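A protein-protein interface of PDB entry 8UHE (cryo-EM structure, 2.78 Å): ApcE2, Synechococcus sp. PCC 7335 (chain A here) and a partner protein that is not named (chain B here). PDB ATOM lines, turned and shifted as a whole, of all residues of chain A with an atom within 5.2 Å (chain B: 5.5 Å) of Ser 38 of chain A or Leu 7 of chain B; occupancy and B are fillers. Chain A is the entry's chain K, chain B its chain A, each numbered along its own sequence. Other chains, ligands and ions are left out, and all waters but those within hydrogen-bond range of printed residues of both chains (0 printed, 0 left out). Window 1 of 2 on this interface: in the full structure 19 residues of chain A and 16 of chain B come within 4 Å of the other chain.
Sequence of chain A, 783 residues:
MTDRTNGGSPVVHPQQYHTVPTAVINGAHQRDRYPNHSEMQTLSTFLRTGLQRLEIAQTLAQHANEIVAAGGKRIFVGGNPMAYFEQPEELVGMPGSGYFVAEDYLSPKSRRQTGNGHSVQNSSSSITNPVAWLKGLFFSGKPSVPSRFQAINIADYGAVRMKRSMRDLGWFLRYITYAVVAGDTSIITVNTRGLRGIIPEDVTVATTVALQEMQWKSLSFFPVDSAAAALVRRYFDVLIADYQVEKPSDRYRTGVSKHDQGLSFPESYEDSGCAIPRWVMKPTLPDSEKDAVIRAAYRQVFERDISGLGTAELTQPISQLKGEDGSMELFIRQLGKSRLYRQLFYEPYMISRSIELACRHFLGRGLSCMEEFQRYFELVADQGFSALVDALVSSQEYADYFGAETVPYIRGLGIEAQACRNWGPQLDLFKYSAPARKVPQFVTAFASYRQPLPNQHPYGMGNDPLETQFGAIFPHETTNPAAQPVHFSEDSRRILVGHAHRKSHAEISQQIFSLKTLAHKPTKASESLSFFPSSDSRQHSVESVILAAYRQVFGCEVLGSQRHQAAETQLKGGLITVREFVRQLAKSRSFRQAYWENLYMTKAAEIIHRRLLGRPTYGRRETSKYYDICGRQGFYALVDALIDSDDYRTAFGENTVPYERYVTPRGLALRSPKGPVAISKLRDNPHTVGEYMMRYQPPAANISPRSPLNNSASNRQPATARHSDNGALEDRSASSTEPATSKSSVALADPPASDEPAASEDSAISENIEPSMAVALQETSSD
The side-chain carboxylate (OE2) of Glu 6 of chain B is in hydrogen-bond range of the side-chain amide nitrogen (ND2) of Asn 36 of chain A, at 3.2 Å.
OE1 of Glu 6 of chain B is in hydrogen-bond range of OG of Ser 38 of chain A, at 2.4 Å.
The backbone carbonyl oxygen (O) of Glu 39 of chain A sits close to the side-chain hydroxyl (OG1) of Thr 42 of chain A (3.3 Å).
OD1 of Asn 36 of chain A lies close to OE1 of Glu 39 of chain A, at 3.0 Å.
The backbone carbonyl oxygen of Leu 7 of chain B is in hydrogen-bond range of the side-chain hydroxyl of Ser 10 of chain B (2.9 Å).
The side-chain hydroxyl (OG1) of Thr 42 of chain A sits at hydrogen-bond distance from the backbone carbonyl oxygen (O) of Ser 38 of chain A.
The side-chain hydroxyl (OG) of Ser 10 of chain B is in hydrogen-bond range of the side-chain carboxylate (OE2) of Glu 22 of chain B (3.1 Å).
O of Glu 6 of chain B is in hydrogen-bond range of OG of Ser 10 of chain B, 2.7 Å away.
CD2 of Leu 7 of chain B touches OG of Ser 38 of chain A (3.9 Å).
CD1 of Ile 25 of chain B touches O of Ser 38 of chain A, at 3.2 Å.
Leu 3 of chain B touches Gln 41 of chain A (CD1 to OE1, 3.7 Å).
CG2 of Ile 25 of chain B touches OE1 of Gln 41 of chain A, 3.7 Å away.
Thr 42 of chain A touches Glu 22 of chain B (OG1 to OE1, 3.8 Å).
Thr 42 of chain A touches Ile 25 of chain B.
Met 40 of chain A touches none of the printed residues of chain B.
Of the printed residues of chain A, Leu 3 of chain B touches Gln 41 (3.7 Å).
Printed residues of chain A within 4 Å of Glu 6 of chain B: Asn 36 (3.2 Å) and Ser 38 (2.4 Å).
Leu 7 of chain B touches one residue of chain A.
Phe 26 of chain B touches none of the printed residues of chain A.
Of the 15 printed residues of chain B, 5 touch a printed residue of chain A.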
ATOM      1  N   ASN A  36      19.805 -24.532   2.415  1.00  0.00           N
ATOM      2  CA  ASN A  36      21.119 -23.917   2.377  1.00  0.00           C
ATOM      3  C   ASN A  36      22.190 -24.953   2.044  1.00  0.00           C
ATOM      4  O   ASN A  36      21.893 -26.095   1.685  1.00  0.00           O
ATOM      5  CB  ASN A  36      21.407 -23.193   3.693  1.00  0.00           C
ATOM      6  CG  ASN A  36      20.884 -23.940   4.896  1.00  0.00           C
ATOM      7  OD1 ASN A  36      19.873 -24.632   4.821  1.00  0.00           O
ATOM      8  ND2 ASN A  36      21.556 -23.778   6.026  1.00  0.00           N
ATOM      9  N   HIS A  37      23.452 -24.525   2.142  1.00  0.00           N
ATOM     10  CA  HIS A  37      24.564 -25.319   1.626  1.00  0.00           C
ATOM     11  C   HIS A  37      24.733 -26.631   2.379  1.00  0.00           C
ATOM     12  O   HIS A  37      25.083 -27.652   1.782  1.00  0.00           O
ATOM     13  CB  HIS A  37      25.857 -24.509   1.674  1.00  0.00           C
ATOM     14  CG  HIS A  37      25.645 -23.040   1.506  1.00  0.00           C
ATOM     15  ND1 HIS A  37      25.778 -22.146   2.546  1.00  0.00           N
ATOM     16  CD2 HIS A  37      25.293 -22.310   0.422  1.00  0.00           C
ATOM     17  CE1 HIS A  37      25.526 -20.926   2.107  1.00  0.00           C
ATOM     18  NE2 HIS A  37      25.229 -20.998   0.821  1.00  0.00           N
ATOM     19  N   SER A  38      24.501 -26.630   3.693  1.00  0.00           N
ATOM     20  CA  SER A  38      24.595 -27.897   4.409  1.00  0.00           C
ATOM     21  C   SER A  38      23.392 -28.791   4.159  1.00  0.00           C
ATOM     22  O   SER A  38      23.552 -30.010   4.110  1.00  0.00           O
ATOM     23  CB  SER A  38      24.758 -27.684   5.904  1.00  0.00           C
ATOM     24  OG  SER A  38      23.508 -27.819   6.559  1.00  0.00           O
ATOM     25  N   GLU A  39      22.199 -28.227   3.992  1.00  0.00           N
ATOM     26  CA  GLU A  39      21.065 -29.033   3.552  1.00  0.00           C
ATOM     27  C   GLU A  39      21.247 -29.513   2.129  1.00  0.00           C
ATOM     28  O   GLU A  39      20.844 -30.640   1.772  1.00  0.00           O
ATOM     29  CB  GLU A  39      19.768 -28.236   3.700  1.00  0.00           C
ATOM     30  CG  GLU A  39      19.249 -28.233   5.133  1.00  0.00           C
ATOM     31  CD  GLU A  39      18.185 -27.188   5.383  1.00  0.00           C
ATOM     32  OE1 GLU A  39      17.656 -26.625   4.405  1.00  0.00           O
ATOM     33  OE2 GLU A  39      17.892 -26.910   6.564  1.00  0.00           O
ATOM     34  N   MET A  40      21.918 -28.685   1.340  1.00  0.00           N
ATOM     35  CA  MET A  40      22.303 -29.112   0.006  1.00  0.00           C
ATOM     36  C   MET A  40      23.276 -30.271   0.036  1.00  0.00           C
ATOM     37  O   MET A  40      23.186 -31.202  -0.776  1.00  0.00           O
ATOM     38  CB  MET A  40      22.871 -27.941  -0.812  1.00  0.00           C
ATOM     39  CG  MET A  40      21.809 -27.076  -1.521  1.00  0.00           C
ATOM     40  SD  MET A  40      20.285 -27.850  -2.110  1.00  0.00           S
ATOM     41  CE  MET A  40      20.717 -29.497  -2.781  1.00  0.00           C
ATOM     42  N   GLN A  41      24.215 -30.215   0.966  1.00  0.00           N
ATOM     43  CA  GLN A  41      25.160 -31.290   1.123  1.00  0.00           C
ATOM     44  C   GLN A  41      24.486 -32.531   1.679  1.00  0.00           C
ATOM     45  O   GLN A  41      24.888 -33.638   1.327  1.00  0.00           O
ATOM     46  CB  GLN A  41      26.316 -30.827   2.009  1.00  0.00           C
ATOM     47  CG  GLN A  41      27.514 -30.338   1.196  1.00  0.00           C
ATOM     48  CD  GLN A  41      28.599 -29.712   2.046  1.00  0.00           C
ATOM     49  OE1 GLN A  41      28.712 -29.995   3.237  1.00  0.00           O
ATOM     50  NE2 GLN A  41      29.409 -28.855   1.433  1.00  0.00           N
ATOM     51  N   THR A  42      23.439 -32.364   2.497  1.00  0.00           N
ATOM     52  CA  THR A  42      22.630 -33.500   2.935  1.00  0.00           C
ATOM     53  C   THR A  42      22.048 -34.239   1.743  1.00  0.00           C
ATOM     54  O   THR A  42      22.246 -35.452   1.584  1.00  0.00           O
ATOM     55  CB  THR A  42      21.469 -33.043   3.820  1.00  0.00           C
ATOM     56  OG1 THR A  42      21.843 -31.910   4.600  1.00  0.00           O
ATOM     57  CG2 THR A  42      21.052 -34.155   4.733  1.00  0.00           C
ATOM     58  N   SER B   2      28.668 -20.335  10.691  1.00  0.00           N
ATOM     59  CA  SER B   2      29.359 -21.349   9.904  1.00  0.00           C
ATOM     60  C   SER B   2      28.432 -22.521   9.601  1.00  0.00           C
ATOM     61  O   SER B   2      27.298 -22.564  10.081  1.00  0.00           O
ATOM     62  CB  SER B   2      30.609 -21.838  10.637  1.00  0.00           C
ATOM     63  OG  SER B   2      30.298 -22.861  11.565  1.00  0.00           O
ATOM     64  N   LEU B   3      28.919 -23.455   8.777  1.00  0.00           N
ATOM     65  CA  LEU B   3      28.165 -24.673   8.492  1.00  0.00           C
ATOM     66  C   LEU B   3      27.998 -25.513   9.749  1.00  0.00           C
ATOM     67  O   LEU B   3      26.951 -26.137   9.959  1.00  0.00           O
ATOM     68  CB  LEU B   3      28.866 -25.474   7.386  1.00  0.00           C
ATOM     69  CG  LEU B   3      28.544 -26.947   7.090  1.00  0.00           C
ATOM     70  CD1 LEU B   3      28.743 -27.220   5.614  1.00  0.00           C
ATOM     71  CD2 LEU B   3      29.411 -27.916   7.881  1.00  0.00           C
ATOM     72  N   VAL B   4      29.046 -25.568  10.574  1.00  0.00           N
ATOM     73  CA  VAL B   4      29.003 -26.299  11.836  1.00  0.00           C
ATOM     74  C   VAL B   4      27.931 -25.743  12.754  1.00  0.00           C
ATOM     75  O   VAL B   4      27.126 -26.497  13.323  1.00  0.00           O
ATOM     76  CB  VAL B   4      30.389 -26.246  12.497  1.00  0.00           C
ATOM     77  CG1 VAL B   4      30.431 -27.094  13.719  1.00  0.00           C
ATOM     78  CG2 VAL B   4      31.452 -26.644  11.482  1.00  0.00           C
ATOM     79  N   THR B   5      27.893 -24.415  12.896  1.00  0.00           N
ATOM     80  CA  THR B   5      26.886 -23.785  13.739  1.00  0.00           C
ATOM     81  C   THR B   5      25.486 -24.083  13.233  1.00  0.00           C
ATOM     82  O   THR B   5      24.604 -24.429  14.018  1.00  0.00           O
ATOM     83  CB  THR B   5      27.103 -22.272  13.821  1.00  0.00           C
ATOM     84  OG1 THR B   5      27.015 -21.695  12.512  1.00  0.00           O
ATOM     85  CG2 THR B   5      28.447 -21.951  14.439  1.00  0.00           C
ATOM     86  N   GLU B   6      25.276 -23.998  11.918  1.00  0.00           N
ATOM     87  CA  GLU B   6      23.929 -24.181  11.386  1.00  0.00           C
ATOM     88  C   GLU B   6      23.483 -25.639  11.491  1.00  0.00           C
ATOM     89  O   GLU B   6      22.302 -25.911  11.748  1.00  0.00           O
ATOM     90  CB  GLU B   6      23.874 -23.660   9.948  1.00  0.00           C
ATOM     91  CG  GLU B   6      22.770 -24.230   9.107  1.00  0.00           C
ATOM     92  CD  GLU B   6      23.252 -25.359   8.256  1.00  0.00           C
ATOM     93  OE1 GLU B   6      22.784 -26.497   8.469  1.00  0.00           O
ATOM     94  OE2 GLU B   6      24.093 -25.098   7.376  1.00  0.00           O
ATOM     95  N   LEU B   7      24.418 -26.585  11.330  1.00  0.00           N
ATOM     96  CA  LEU B   7      24.142 -27.991  11.630  1.00  0.00           C
ATOM     97  C   LEU B   7      23.676 -28.164  13.069  1.00  0.00           C
ATOM     98  O   LEU B   7      22.693 -28.866  13.344  1.00  0.00           O
ATOM     99  CB  LEU B   7      25.395 -28.838  11.404  1.00  0.00           C
ATOM    100  CG  LEU B   7      25.863 -29.217  10.004  1.00  0.00           C
ATOM    101  CD1 LEU B   7      27.182 -29.872  10.096  1.00  0.00           C
ATOM    102  CD2 LEU B   7      24.878 -30.139   9.334  1.00  0.00           C
ATOM    103  N   ILE B   8      24.380 -27.516  14.003  1.00  0.00           N
ATOM    104  CA  ILE B   8      24.031 -27.627  15.417  1.00  0.00           C
ATOM    105  C   ILE B   8      22.668 -26.994  15.697  1.00  0.00           C
ATOM    106  O   ILE B   8      21.860 -27.548  16.447  1.00  0.00           O
ATOM    107  CB  ILE B   8      25.148 -27.015  16.283  1.00  0.00           C
ATOM    108  CG1 ILE B   8      26.442 -27.822  16.123  1.00  0.00           C
ATOM    109  CG2 ILE B   8      24.733 -26.918  17.736  1.00  0.00           C
ATOM    110  CD1 ILE B   8      26.494 -29.098  16.925  1.00  0.00           C
ATOM    111  N   LEU B   9      22.379 -25.842  15.081  1.00  0.00           N
ATOM    112  CA  LEU B   9      21.100 -25.169  15.305  1.00  0.00           C
ATOM    113  C   LEU B   9      19.936 -25.956  14.715  1.00  0.00           C
ATOM    114  O   LEU B   9      18.831 -25.944  15.270  1.00  0.00           O
ATOM    115  CB  LEU B   9      21.110 -23.762  14.708  1.00  0.00           C
ATOM    116  CG  LEU B   9      22.197 -22.776  15.120  1.00  0.00           C
ATOM    117  CD1 LEU B   9      22.476 -21.813  13.976  1.00  0.00           C
ATOM    118  CD2 LEU B   9      21.846 -22.039  16.383  1.00  0.00           C
ATOM    119  N   SER B  10      20.148 -26.610  13.572  1.00  0.00           N
ATOM    120  CA  SER B  10      19.087 -27.432  13.003  1.00  0.00           C
ATOM    121  C   SER B  10      18.881 -28.707  13.809  1.00  0.00           C
ATOM    122  O   SER B  10      17.751 -29.192  13.914  1.00  0.00           O
ATOM    123  CB  SER B  10      19.397 -27.768  11.547  1.00  0.00           C
ATOM    124  OG  SER B  10      20.770 -28.067  11.389  1.00  0.00           O
ATOM    125  N   ALA B  11      19.953 -29.268  14.380  1.00  0.00           N
ATOM    126  CA  ALA B  11      19.775 -30.356  15.335  1.00  0.00           C
ATOM    127  C   ALA B  11      19.112 -29.863  16.614  1.00  0.00           C
ATOM    128  O   ALA B  11      18.483 -30.646  17.334  1.00  0.00           O
ATOM    129  CB  ALA B  11      21.119 -31.008  15.651  1.00  0.00           C
ATOM    130  N   ASP B  12      19.269 -28.581  16.918  1.00  0.00           N
ATOM    131  CA  ASP B  12      18.532 -27.928  17.987  1.00  0.00           C
ATOM    132  C   ASP B  12      17.200 -27.454  17.419  1.00  0.00           C
ATOM    133  O   ASP B  12      16.845 -27.774  16.281  1.00  0.00           O
ATOM    134  CB  ASP B  12      19.354 -26.785  18.571  1.00  0.00           C
ATOM    135  CG  ASP B  12      19.170 -26.647  20.057  1.00  0.00           C
ATOM    136  OD1 ASP B  12      18.025 -26.408  20.495  1.00  0.00           O
ATOM    137  OD2 ASP B  12      20.174 -26.768  20.787  1.00  0.00           O
ATOM    138  N   PRO B  18      22.225 -34.535  16.310  1.00  0.00           N
ATOM    139  CA  PRO B  18      22.615 -34.361  14.906  1.00  0.00           C
ATOM    140  C   PRO B  18      22.543 -35.696  14.187  1.00  0.00           C
ATOM    141  O   PRO B  18      23.170 -36.677  14.594  1.00  0.00           O
ATOM    142  CB  PRO B  18      24.046 -33.823  14.999  1.00  0.00           C
ATOM    143  CG  PRO B  18      24.111 -33.188  16.344  1.00  0.00           C
ATOM    144  CD  PRO B  18      23.257 -34.031  17.230  1.00  0.00           C
ATOM    145  N   GLU B  22      23.699 -35.263   8.942  1.00  0.00           N
ATOM    146  CA  GLU B  22      24.369 -34.047   9.401  1.00  0.00           C
ATOM    147  C   GLU B  22      25.830 -34.321   9.747  1.00  0.00           C
ATOM    148  O   GLU B  22      26.716 -33.505   9.469  1.00  0.00           O
ATOM    149  CB  GLU B  22      23.631 -33.464  10.609  1.00  0.00           C
ATOM    150  CG  GLU B  22      22.150 -33.177  10.383  1.00  0.00           C
ATOM    151  CD  GLU B  22      21.910 -31.891   9.614  1.00  0.00           C
ATOM    152  OE1 GLU B  22      22.009 -31.907   8.369  1.00  0.00           O
ATOM    153  OE2 GLU B  22      21.637 -30.857  10.258  1.00  0.00           O
ATOM    154  N   ILE B  25      27.775 -34.559   6.605  1.00  0.00           N
ATOM    155  CA  ILE B  25      28.056 -33.185   6.189  1.00  0.00           C
ATOM    156  C   ILE B  25      29.295 -32.692   6.917  1.00  0.00           C
ATOM    157  O   ILE B  25      30.200 -32.105   6.311  1.00  0.00           O
ATOM    158  CB  ILE B  25      26.866 -32.264   6.503  1.00  0.00           C
ATOM    159  CG1 ILE B  25      25.764 -32.425   5.481  1.00  0.00           C
ATOM    160  CG2 ILE B  25      27.281 -30.803   6.546  1.00  0.00           C
ATOM    161  CD1 ILE B  25      24.467 -32.341   6.145  1.00  0.00           C
ATOM    162  N   PHE B  26      29.310 -32.912   8.231  1.00  0.00           N
ATOM    163  CA  PHE B  26      30.430 -32.596   9.106  1.00  0.00           C
ATOM    164  C   PHE B  26      31.746 -33.174   8.605  1.00  0.00           C
ATOM    165  O   PHE B  26      32.706 -32.440   8.344  1.00  0.00           O
ATOM    166  CB  PHE B  26      30.146 -33.135  10.504  1.00  0.00           C
ATOM    167  CG  PHE B  26      30.492 -32.191  11.599  1.00  0.00           C
ATOM    168  CD1 PHE B  26      31.600 -32.412  12.384  1.00  0.00           C
ATOM    169  CD2 PHE B  26      29.719 -31.104  11.856  1.00  0.00           C
ATOM    170  CE1 PHE B  26      31.924 -31.543  13.393  1.00  0.00           C
ATOM    171  CE2 PHE B  26      30.010 -30.264  12.840  1.00  0.00           C
ATOM    172  CZ  PHE B  26      31.128 -30.465  13.620  1.00  0.00           C
